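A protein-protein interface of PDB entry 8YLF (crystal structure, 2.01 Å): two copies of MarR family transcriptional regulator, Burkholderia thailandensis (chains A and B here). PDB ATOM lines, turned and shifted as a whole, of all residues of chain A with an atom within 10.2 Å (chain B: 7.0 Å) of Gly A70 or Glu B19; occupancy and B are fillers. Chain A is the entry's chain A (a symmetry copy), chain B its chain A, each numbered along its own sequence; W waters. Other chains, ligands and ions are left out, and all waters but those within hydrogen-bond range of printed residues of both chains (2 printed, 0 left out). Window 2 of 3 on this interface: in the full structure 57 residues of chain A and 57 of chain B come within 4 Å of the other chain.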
ATOM      1  N   VAL A  62      11.264 -29.634  16.115  1.00  0.00           N
ATOM      2  CA  VAL A  62      11.865 -30.741  16.851  1.00  0.00           C
ATOM      3  C   VAL A  62      13.067 -30.252  17.631  1.00  0.00           C
ATOM      4  O   VAL A  62      13.183 -30.488  18.838  1.00  0.00           O
ATOM      5  CB  VAL A  62      12.250 -31.888  15.901  1.00  0.00           C
ATOM      6  CG1 VAL A  62      13.167 -32.867  16.627  1.00  0.00           C
ATOM      7  CG2 VAL A  62      11.002 -32.602  15.417  1.00  0.00           C
ATOM      8  N   LEU A  63      13.977 -29.539  16.955  1.00  0.00           N
ATOM      9  CA  LEU A  63      15.169 -29.054  17.642  1.00  0.00           C
ATOM     10  C   LEU A  63      14.802 -28.073  18.749  1.00  0.00           C
ATOM     11  O   LEU A  63      15.353 -28.135  19.857  1.00  0.00           O
ATOM     12  CB  LEU A  63      16.128 -28.400  16.643  1.00  0.00           C
ATOM     13  CG  LEU A  63      16.655 -29.209  15.446  1.00  0.00           C
ATOM     14  CD1 LEU A  63      17.777 -28.383  14.739  1.00  0.00           C
ATOM     15  CD2 LEU A  63      17.199 -30.554  15.880  1.00  0.00           C
ATOM     16  N   ALA A  64      13.868 -27.159  18.470  1.00  0.00           N
ATOM     17  CA  ALA A  64      13.453 -26.202  19.492  1.00  0.00           C
ATOM     18  C   ALA A  64      12.813 -26.907  20.680  1.00  0.00           C
ATOM     19  O   ALA A  64      13.029 -26.522  21.834  1.00  0.00           O
ATOM     20  CB  ALA A  64      12.477 -25.190  18.896  1.00  0.00           C
ATOM     21  N   THR A  65      12.022 -27.939  20.419  1.00  0.00           N
ATOM     22  CA  THR A  65      11.386 -28.655  21.518  1.00  0.00           C
ATOM     23  C   THR A  65      12.420 -29.354  22.393  1.00  0.00           C
ATOM     24  O   THR A  65      12.339 -29.293  23.624  1.00  0.00           O
ATOM     25  CB  THR A  65      10.369 -29.631  20.953  1.00  0.00           C
ATOM     26  OG1 THR A  65       9.409 -28.878  20.200  1.00  0.00           O
ATOM     27  CG2 THR A  65       9.650 -30.414  22.077  1.00  0.00           C
ATOM     28  N   LEU A  66      13.426 -29.980  21.777  1.00  0.00           N
ATOM     29  CA  LEU A  66      14.471 -30.641  22.554  1.00  0.00           C
ATOM     30  C   LEU A  66      15.261 -29.630  23.368  1.00  0.00           C
ATOM     31  O   LEU A  66      15.499 -29.833  24.565  1.00  0.00           O
ATOM     32  CB  LEU A  66      15.397 -31.436  21.629  1.00  0.00           C
ATOM     33  CG  LEU A  66      14.713 -32.601  20.900  1.00  0.00           C
ATOM     34  CD1 LEU A  66      15.533 -33.116  19.730  1.00  0.00           C
ATOM     35  CD2 LEU A  66      14.486 -33.725  21.889  1.00  0.00           C
ATOM     36  N   ARG A  67      15.670 -28.523  22.735  1.00  0.00           N
ATOM     37  CA  ARG A  67      16.455 -27.512  23.437  1.00  0.00           C
ATOM     38  C   ARG A  67      15.697 -26.962  24.635  1.00  0.00           C
ATOM     39  O   ARG A  67      16.251 -26.846  25.735  1.00  0.00           O
ATOM     40  CB  ARG A  67      16.827 -26.373  22.487  1.00  0.00           C
ATOM     41  CG  ARG A  67      17.493 -25.188  23.186  1.00  0.00           C
ATOM     42  CD  ARG A  67      18.928 -25.522  23.611  1.00  0.00           C
ATOM     43  NE  ARG A  67      19.570 -24.434  24.356  1.00  0.00           N
ATOM     44  CZ  ARG A  67      19.301 -24.171  25.631  1.00  0.00           C
ATOM     45  NH1 ARG A  67      18.391 -24.904  26.290  1.00  0.00           N
ATOM     46  NH2 ARG A  67      19.920 -23.181  26.250  1.00  0.00           N
ATOM     47  N   ARG A  68      14.426 -26.598  24.445  1.00  0.00           N
ATOM     48  CA  ARG A  68      13.766 -25.937  25.558  1.00  0.00           C
ATOM     49  C   ARG A  68      13.330 -26.916  26.628  1.00  0.00           C
ATOM     50  O   ARG A  68      12.919 -26.482  27.708  1.00  0.00           O
ATOM     51  CB  ARG A  68      12.571 -25.106  25.083  1.00  0.00           C
ATOM     52  CG  ARG A  68      11.422 -25.877  24.529  1.00  0.00           C
ATOM     53  CD  ARG A  68      10.280 -24.926  24.196  1.00  0.00           C
ATOM     54  NE  ARG A  68       9.572 -25.369  23.005  1.00  0.00           N
ATOM     55  CZ  ARG A  68       8.581 -26.259  23.014  1.00  0.00           C
ATOM     56  NH1 ARG A  68       8.162 -26.788  24.160  1.00  0.00           N
ATOM     57  NH2 ARG A  68       8.011 -26.615  21.870  1.00  0.00           N
ATOM     58  N   SER A  69      13.444 -28.220  26.379  1.00  0.00           N
ATOM     59  CA  SER A  69      13.167 -29.159  27.456  1.00  0.00           C
ATOM     60  C   SER A  69      14.286 -29.193  28.485  1.00  0.00           C
ATOM     61  O   SER A  69      14.152 -29.899  29.487  1.00  0.00           O
ATOM     62  CB  SER A  69      12.929 -30.564  26.890  1.00  0.00           C
ATOM     63  OG  SER A  69      14.149 -31.120  26.414  1.00  0.00           O
ATOM     64  N   GLY A  70      15.379 -28.465  28.260  1.00  0.00           N
ATOM     65  CA  GLY A  70      16.473 -28.406  29.207  1.00  0.00           C
ATOM     66  C   GLY A  70      17.443 -29.568  29.059  1.00  0.00           C
ATOM     67  O   GLY A  70      17.141 -30.609  28.476  1.00  0.00           O
ATOM     68  N   ALA A  71      18.636 -29.374  29.612  1.00  0.00           N
ATOM     69  CA  ALA A  71      19.675 -30.384  29.498  1.00  0.00           C
ATOM     70  C   ALA A  71      19.199 -31.689  30.133  1.00  0.00           C
ATOM     71  O   ALA A  71      18.480 -31.661  31.141  1.00  0.00           O
ATOM     72  CB  ALA A  71      20.967 -29.904  30.163  1.00  0.00           C
ATOM     73  N   PRO A  72      19.569 -32.855  29.573  1.00  0.00           N
ATOM     74  CA  PRO A  72      20.439 -33.084  28.410  1.00  0.00           C
ATOM     75  C   PRO A  72      19.743 -32.965  27.055  1.00  0.00           C
ATOM     76  O   PRO A  72      20.274 -33.495  26.076  1.00  0.00           O
ATOM     77  CB  PRO A  72      20.909 -34.524  28.618  1.00  0.00           C
ATOM     78  CG  PRO A  72      19.734 -35.176  29.264  1.00  0.00           C
ATOM     79  CD  PRO A  72      19.124 -34.129  30.171  1.00  0.00           C
ATOM     80  N   TYR A  73      18.576 -32.313  27.006  1.00  0.00           N
ATOM     81  CA  TYR A  73      17.878 -32.047  25.746  1.00  0.00           C
ATOM     82  C   TYR A  73      17.496 -33.353  25.064  1.00  0.00           C
ATOM     83  O   TYR A  73      17.730 -33.546  23.869  1.00  0.00           O
ATOM     84  CB  TYR A  73      18.729 -31.181  24.804  1.00  0.00           C
ATOM     85  CG  TYR A  73      19.513 -30.094  25.497  1.00  0.00           C
ATOM     86  CD1 TYR A  73      18.876 -28.985  26.039  1.00  0.00           C
ATOM     87  CD2 TYR A  73      20.898 -30.174  25.600  1.00  0.00           C
ATOM     88  CE1 TYR A  73      19.606 -27.980  26.686  1.00  0.00           C
ATOM     89  CE2 TYR A  73      21.630 -29.184  26.235  1.00  0.00           C
ATOM     90  CZ  TYR A  73      20.982 -28.089  26.777  1.00  0.00           C
ATOM     91  OH  TYR A  73      21.716 -27.109  27.413  1.00  0.00           O
ATOM     92  N   ALA A  74      16.900 -34.256  25.841  1.00  0.00           N
ATOM     93  CA  ALA A  74      16.566 -35.594  25.383  1.00  0.00           C
ATOM     94  C   ALA A  74      15.132 -35.921  25.783  1.00  0.00           C
ATOM     95  O   ALA A  74      14.766 -35.794  26.956  1.00  0.00           O
ATOM     96  CB  ALA A  74      17.535 -36.628  25.974  1.00  0.00           C
ATOM     97  N   LEU A  75      14.322 -36.326  24.809  1.00  0.00           N
ATOM     98  CA  LEU A  75      12.933 -36.682  25.069  1.00  0.00           C
ATOM     99  C   LEU A  75      12.575 -37.932  24.291  1.00  0.00           C
ATOM    100  O   LEU A  75      13.099 -38.167  23.199  1.00  0.00           O
ATOM    101  CB  LEU A  75      11.966 -35.568  24.646  1.00  0.00           C
ATOM    102  CG  LEU A  75      12.140 -34.159  25.200  1.00  0.00           C
ATOM    103  CD1 LEU A  75      11.291 -33.197  24.389  1.00  0.00           C
ATOM    104  CD2 LEU A  75      11.704 -34.169  26.674  1.00  0.00           C
ATOM    105  N   ALA A  83       5.175 -31.943  23.392  1.00  0.00           N
ATOM    106  CA  ALA A  83       5.789 -30.663  23.749  1.00  0.00           C
ATOM    107  C   ALA A  83       6.024 -29.762  22.551  1.00  0.00           C
ATOM    108  O   ALA A  83       6.481 -28.618  22.735  1.00  0.00           O
ATOM    109  CB  ALA A  83       7.111 -30.893  24.485  1.00  0.00           C
ATOM    110  N   VAL A 118      15.365 -39.233  21.918  1.00  0.00           N
ATOM    111  CA  VAL A 118      15.894 -38.363  20.873  1.00  0.00           C
ATOM    112  C   VAL A 118      16.581 -37.201  21.578  1.00  0.00           C
ATOM    113  O   VAL A 118      15.965 -36.520  22.404  1.00  0.00           O
ATOM    114  CB  VAL A 118      14.786 -37.880  19.922  1.00  0.00           C
ATOM    115  CG1 VAL A 118      15.342 -36.906  18.880  1.00  0.00           C
ATOM    116  CG2 VAL A 118      14.124 -39.068  19.240  1.00  0.00           C
ATOM    117  N   ALA A 119      17.862 -36.992  21.281  1.00  0.00           N
ATOM    118  CA  ALA A 119      18.659 -35.981  21.967  1.00  0.00           C
ATOM    119  C   ALA A 119      19.372 -35.103  20.951  1.00  0.00           C
ATOM    120  O   ALA A 119      19.812 -35.598  19.911  1.00  0.00           O
ATOM    121  CB  ALA A 119      19.699 -36.629  22.912  1.00  0.00           C
ATOM    122  N   LEU A 120      19.494 -33.805  21.261  1.00  0.00           N
ATOM    123  CA  LEU A 120      20.331 -32.919  20.458  1.00  0.00           C
ATOM    124  C   LEU A 120      21.762 -33.408  20.456  1.00  0.00           C
ATOM    125  O   LEU A 120      22.290 -33.835  21.486  1.00  0.00           O
ATOM    126  CB  LEU A 120      20.321 -31.487  21.003  1.00  0.00           C
ATOM    127  CG  LEU A 120      19.041 -30.683  20.836  1.00  0.00           C
ATOM    128  CD1 LEU A 120      19.162 -29.377  21.591  1.00  0.00           C
ATOM    129  CD2 LEU A 120      18.778 -30.444  19.356  1.00  0.00           C
ATOM    130  N   ARG A 125      22.475 -28.589  19.040  1.00  0.00           N
ATOM    131  CA  ARG A 125      22.216 -27.576  20.057  1.00  0.00           C
ATOM    132  C   ARG A 125      22.745 -26.212  19.626  1.00  0.00           C
ATOM    133  O   ARG A 125      22.068 -25.189  19.796  1.00  0.00           O
ATOM    134  CB  ARG A 125      22.845 -27.978  21.384  1.00  0.00           C
ATOM    135  CG  ARG A 125      22.620 -26.919  22.427  1.00  0.00           C
ATOM    136  CD  ARG A 125      23.457 -27.142  23.658  1.00  0.00           C
ATOM    137  NE  ARG A 125      23.415 -25.964  24.513  1.00  0.00           N
ATOM    138  CZ  ARG A 125      24.151 -25.814  25.603  1.00  0.00           C
ATOM    139  NH1 ARG A 125      25.001 -26.767  25.962  1.00  0.00           N
ATOM    140  NH2 ARG A 125      24.046 -24.705  26.319  1.00  0.00           N
ATOM    141  N   ILE A 128      20.267 -24.738  16.886  1.00  0.00           N
ATOM    142  CA  ILE A 128      18.989 -24.204  17.353  1.00  0.00           C
ATOM    143  C   ILE A 128      19.184 -23.018  18.299  1.00  0.00           C
ATOM    144  O   ILE A 128      18.331 -22.118  18.350  1.00  0.00           O
ATOM    145  CB  ILE A 128      18.141 -25.328  17.997  1.00  0.00           C
ATOM    146  CG1 ILE A 128      16.703 -24.856  18.178  1.00  0.00           C
ATOM    147  CG2 ILE A 128      18.732 -25.804  19.333  1.00  0.00           C
ATOM    148  CD1 ILE A 128      16.055 -24.505  16.852  1.00  0.00           C
ATOM    149  N   ASP A 129      20.296 -22.982  19.050  1.00  0.00           N
ATOM    150  CA  ASP A 129      20.638 -21.800  19.845  1.00  0.00           C
ATOM    151  C   ASP A 129      20.843 -20.570  18.956  1.00  0.00           C
ATOM    152  O   ASP A 129      20.433 -19.461  19.309  1.00  0.00           O
ATOM    153  CB  ASP A 129      21.910 -22.056  20.666  1.00  0.00           C
ATOM    154  CG  ASP A 129      21.635 -22.717  22.016  1.00  0.00           C
ATOM    155  OD1 ASP A 129      20.484 -22.682  22.483  1.00  0.00           O
ATOM    156  OD2 ASP A 129      22.596 -23.238  22.629  1.00  0.00           O
ATOM    157  N   VAL A 132      17.070 -19.927  16.993  1.00  0.00           N
ATOM    158  CA  VAL A 132      15.908 -19.437  17.730  1.00  0.00           C
ATOM    159  C   VAL A 132      15.968 -17.919  17.917  1.00  0.00           C
ATOM    160  O   VAL A 132      14.926 -17.253  17.959  1.00  0.00           O
ATOM    161  CB  VAL A 132      15.752 -20.164  19.077  1.00  0.00           C
ATOM    162  CG1 VAL A 132      16.878 -19.803  20.024  1.00  0.00           C
ATOM    163  CG2 VAL A 132      14.416 -19.821  19.688  1.00  0.00           C
ATOM    164  N   VAL A 133      17.166 -17.344  18.034  1.00  0.00           N
ATOM    165  CA  VAL A 133      17.282 -15.887  18.119  1.00  0.00           C
ATOM    166  C   VAL A 133      16.803 -15.241  16.822  1.00  0.00           C
ATOM    167  O   VAL A 133      16.006 -14.294  16.834  1.00  0.00           O
ATOM    168  CB  VAL A 133      18.726 -15.476  18.453  1.00  0.00           C
ATOM    169  CG1 VAL A 133      18.904 -13.959  18.288  1.00  0.00           C
ATOM    170  CG2 VAL A 133      19.067 -15.889  19.867  1.00  0.00           C
ATOM    171  N   VAL B  13       6.604 -21.146  25.524  1.00  0.00           N
ATOM    172  CA  VAL B  13       7.156 -19.859  25.939  1.00  0.00           C
ATOM    173  C   VAL B  13       7.677 -19.945  27.368  1.00  0.00           C
ATOM    174  O   VAL B  13       8.755 -19.428  27.684  1.00  0.00           O
ATOM    175  CB  VAL B  13       6.097 -18.752  25.780  1.00  0.00           C
ATOM    176  CG1 VAL B  13       6.493 -17.499  26.560  1.00  0.00           C
ATOM    177  CG2 VAL B  13       5.902 -18.432  24.305  1.00  0.00           C
ATOM    178  N   GLU B  14       6.925 -20.608  28.251  1.00  0.00           N
ATOM    179  CA  GLU B  14       7.380 -20.777  29.625  1.00  0.00           C
ATOM    180  C   GLU B  14       8.735 -21.469  29.669  1.00  0.00           C
ATOM    181  O   GLU B  14       9.647 -21.028  30.379  1.00  0.00           O
ATOM    182  CB  GLU B  14       6.348 -21.575  30.425  1.00  0.00           C
ATOM    183  CG  GLU B  14       6.374 -21.310  31.907  1.00  0.00           C
ATOM    184  CD  GLU B  14       5.847 -19.930  32.254  1.00  0.00           C
ATOM    185  OE1 GLU B  14       5.073 -19.358  31.452  1.00  0.00           O
ATOM    186  OE2 GLU B  14       6.215 -19.417  33.328  1.00  0.00           O
ATOM    187  N   GLN B  15       8.886 -22.554  28.909  1.00  0.00           N
ATOM    188  CA  GLN B  15      10.164 -23.254  28.872  1.00  0.00           C
ATOM    189  C   GLN B  15      11.263 -22.368  28.299  1.00  0.00           C
ATOM    190  O   GLN B  15      12.367 -22.313  28.851  1.00  0.00           O
ATOM    191  CB  GLN B  15      10.022 -24.543  28.063  1.00  0.00           C
ATOM    192  CG  GLN B  15       9.090 -25.575  28.707  1.00  0.00           C
ATOM    193  CD  GLN B  15       9.211 -26.938  28.053  1.00  0.00           C
ATOM    194  OE1 GLN B  15       9.224 -27.049  26.827  1.00  0.00           O
ATOM    195  NE2 GLN B  15       9.318 -27.983  28.870  1.00  0.00           N
ATOM    196  N   TRP B  16      10.979 -21.656  27.203  1.00  0.00           N
ATOM    197  CA  TRP B  16      11.996 -20.794  26.598  1.00  0.00           C
ATOM    198  C   TRP B  16      12.432 -19.698  27.561  1.00  0.00           C
ATOM    199  O   TRP B  16      13.628 -19.429  27.711  1.00  0.00           O
ATOM    200  CB  TRP B  16      11.476 -20.181  25.297  1.00  0.00           C
ATOM    201  CG  TRP B  16      11.678 -21.042  24.068  1.00  0.00           C
ATOM    202  CD1 TRP B  16      10.708 -21.489  23.202  1.00  0.00           C
ATOM    203  CD2 TRP B  16      12.928 -21.550  23.568  1.00  0.00           C
ATOM    204  NE1 TRP B  16      11.284 -22.241  22.196  1.00  0.00           N
ATOM    205  CE2 TRP B  16      12.641 -22.295  22.400  1.00  0.00           C
ATOM    206  CE3 TRP B  16      14.258 -21.453  23.998  1.00  0.00           C
ATOM    207  CZ2 TRP B  16      13.637 -22.935  21.660  1.00  0.00           C
ATOM    208  CZ3 TRP B  16      15.251 -22.092  23.259  1.00  0.00           C
ATOM    209  CH2 TRP B  16      14.933 -22.818  22.103  1.00  0.00           C
ATOM    210  N   ARG B  17      11.469 -19.038  28.211  1.00  0.00           N
ATOM    211  CA  ARG B  17      11.808 -18.024  29.205  1.00  0.00           C
ATOM    212  C   ARG B  17      12.722 -18.599  30.278  1.00  0.00           C
ATOM    213  O   ARG B  17      13.654 -17.926  30.739  1.00  0.00           O
ATOM    214  CB  ARG B  17      10.536 -17.448  29.830  1.00  0.00           C
ATOM    215  CG  ARG B  17       9.869 -16.368  28.991  1.00  0.00           C
ATOM    216  CD  ARG B  17       8.487 -16.031  29.516  1.00  0.00           C
ATOM    217  NE  ARG B  17       7.836 -14.997  28.717  1.00  0.00           N
ATOM    218  CZ  ARG B  17       6.523 -14.778  28.704  1.00  0.00           C
ATOM    219  NH1 ARG B  17       5.716 -15.529  29.444  1.00  0.00           N
ATOM    220  NH2 ARG B  17       6.017 -13.816  27.942  1.00  0.00           N
ATOM    221  N   SER B  18      12.485 -19.852  30.668  1.00  0.00           N
ATOM    222  CA  SER B  18      13.350 -20.504  31.645  1.00  0.00           C
ATOM    223  C   SER B  18      14.726 -20.797  31.055  1.00  0.00           C
ATOM    224  O   SER B  18      15.752 -20.527  31.686  1.00  0.00           O
ATOM    225  CB  SER B  18      12.688 -21.789  32.143  1.00  0.00           C
ATOM    226  OG  SER B  18      13.623 -22.615  32.809  1.00  0.00           O
ATOM    227  N   GLU B  19      14.770 -21.325  29.826  1.00  0.00           N
ATOM    228  CA  GLU B  19      16.027 -21.827  29.274  1.00  0.00           C
ATOM    229  C   GLU B  19      16.877 -20.731  28.637  1.00  0.00           C
ATOM    230  O   GLU B  19      18.109 -20.805  28.693  1.00  0.00           O
ATOM    231  CB  GLU B  19      15.758 -22.926  28.244  1.00  0.00           C
ATOM    232  CG  GLU B  19      15.448 -24.291  28.842  1.00  0.00           C
ATOM    233  CD  GLU B  19      16.639 -24.888  29.582  1.00  0.00           C
ATOM    234  OE1 GLU B  19      17.793 -24.710  29.123  1.00  0.00           O
ATOM    235  OE2 GLU B  19      16.415 -25.535  30.630  1.00  0.00           O
ATOM    236  N   ARG B  20      16.250 -19.737  28.011  1.00  0.00           N
ATOM    237  CA  ARG B  20      16.943 -18.663  27.299  1.00  0.00           C
ATOM    238  C   ARG B  20      16.411 -17.334  27.808  1.00  0.00           C
ATOM    239  O   ARG B  20      15.736 -16.599  27.075  1.00  0.00           O
ATOM    240  CB  ARG B  20      16.745 -18.777  25.785  1.00  0.00           C
ATOM    241  CG  ARG B  20      17.472 -19.934  25.111  1.00  0.00           C
ATOM    242  CD  ARG B  20      18.983 -19.798  25.251  1.00  0.00           C
ATOM    243  NE  ARG B  20      19.485 -18.576  24.629  1.00  0.00           N
ATOM    244  CZ  ARG B  20      19.858 -18.471  23.354  1.00  0.00           C
ATOM    245  NH1 ARG B  20      19.774 -19.515  22.536  1.00  0.00           N
ATOM    246  NH2 ARG B  20      20.304 -17.308  22.888  1.00  0.00           N
ATOM    247  N   PRO B  21      16.693 -16.984  29.066  1.00  0.00           N
ATOM    248  CA  PRO B  21      16.189 -15.710  29.596  1.00  0.00           C
ATOM    249  C   PRO B  21      16.710 -14.503  28.836  1.00  0.00           C
ATOM    250  O   PRO B  21      16.140 -13.413  28.963  1.00  0.00           O
ATOM    251  CB  PRO B  21      16.671 -15.720  31.050  1.00  0.00           C
ATOM    252  CG  PRO B  21      17.861 -16.613  31.040  1.00  0.00           C
ATOM    253  CD  PRO B  21      17.575 -17.672  30.027  1.00  0.00           C
ATOM    254  N   ASP B  22      17.767 -14.672  28.042  1.00  0.00           N
ATOM    255  CA  ASP B  22      18.243 -13.627  27.146  1.00  0.00           C
ATOM    256  C   ASP B  22      17.289 -13.382  25.979  1.00  0.00           C
ATOM    257  O   ASP B  22      17.482 -12.406  25.241  1.00  0.00           O
ATOM    258  CB  ASP B  22      19.629 -14.001  26.612  1.00  0.00           C
ATOM    259  CG  ASP B  22      19.609 -15.293  25.797  1.00  0.00           C
ATOM    260  OD1 ASP B  22      19.268 -16.358  26.362  1.00  0.00           O
ATOM    261  OD2 ASP B  22      19.899 -15.238  24.583  1.00  0.00           O
HETATM  262  O   HOH W   1      22.471 -17.549  20.779  1.00  0.00           O
HETATM  263  O   HOH W   2       9.397 -23.505  20.351  1.00  0.00           O
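Water W2 lies within hydrogen-bond range of the indole nitrogen of Trp B16 (2.9 Å) and the guanidinium group of Arg A68 (3.2 Å). Water W1 bridges NH2 of Arg B20 (3.0 Å) and O of Asp A129 (3.2 Å).
No position is printed for both chains.
Along chain A the printed residues that touch a printed residue of chain B span positions 64 to 133. Of the 10 printed residues of chain B, 4 touch a printed residue of chain A. Printed residues of chain B that touch a printed residue of chain A: Gln B15, Trp B16, Glu B19 and Arg B20. Hydrophobic or aromatic side chains of chain B within 4 Å of the printed part of chain A: Trp B16. Among the printed residues, 12 pairs touch across the chains.
NH2 of Arg B20 is in salt-bridge range of OD2 of Asp B22 (2.7 Å). NH2 of Arg A68 is in hydrogen-bond range of OG1 of Thr A65, 3.1 Å away. The guanidinium group (NE) of Arg A67 lies within salt-bridge range of the side-chain carboxylate (OD1) of Asp A129 (2.7 Å). The backbone carbonyl oxygen (O) of Ala A83 is in hydrogen-bond range of the guanidinium group (NH2) of Arg A68. The guanidinium group (NE) of Arg A125 is in salt-bridge range of the side-chain carboxylate (OD2) of Asp A129 (3.4 Å).
Of the printed residues of chain B, Gly A70 touches Glu B19 (3.2 Å). Of the printed residues of chain A, Glu B19 touches Arg A67 (2.9 Å), Arg A68 (3.5 Å) and Gly A70 (3.2 Å). Printed residues of chain B within 4 Å of Val A133: Arg B20. Of the printed residues of chain B, Val A132 touches Trp B16 and Arg B20. Of the printed residues of chain A, Arg B20 touches Arg A67, Asp A129, Val A132 and Val A133. Of the printed residues of chain B, Arg A68 touches Gln B15, Trp B16 and Glu B19. Of the printed residues of chain A, Gln B15 touches Arg A68. Thr A65 touches none of the printed residues of chain B. Leu A66 touches none of the printed residues of chain B. The nearest residue of chain B that does not touch Gly A70 is Gln B15 (6.1 Å). The nearest residue of chain A that does not touch Glu B19 is Tyr A73 (4.5 Å). The nearest printed residue of chain B that does not touch Val A133 is Asp B22 (4.8 Å).
The side-chain amide oxygen of Gln B15 lies within hydrogen-bond range of the guanidinium group of Arg A68, at 2.9 Å. OE1 of Glu B19 is in salt-bridge range of NH1 of Arg A67, 2.9 Å away. NH1 of Arg B20 is in salt-bridge range of OD1 of Asp A129 (3.2 Å).
Among the printed residues, pairs that only touch across the chains: Ala A64 with Trp B16 (3.6 Å), Arg A67 with Trp B16 (3.7 Å), Arg A67 with Arg B20 (3.6 Å), Arg A68 with Trp B16 (3.5 Å), Arg A68 with Glu B19 (3.5 Å), Gly A70 with Glu B19 (3.2 Å), Val A132 with Trp B16 (3.8 Å), Val A132 with Arg B20 (3.8 Å) and Val A133 with Arg B20 (3.6 Å).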
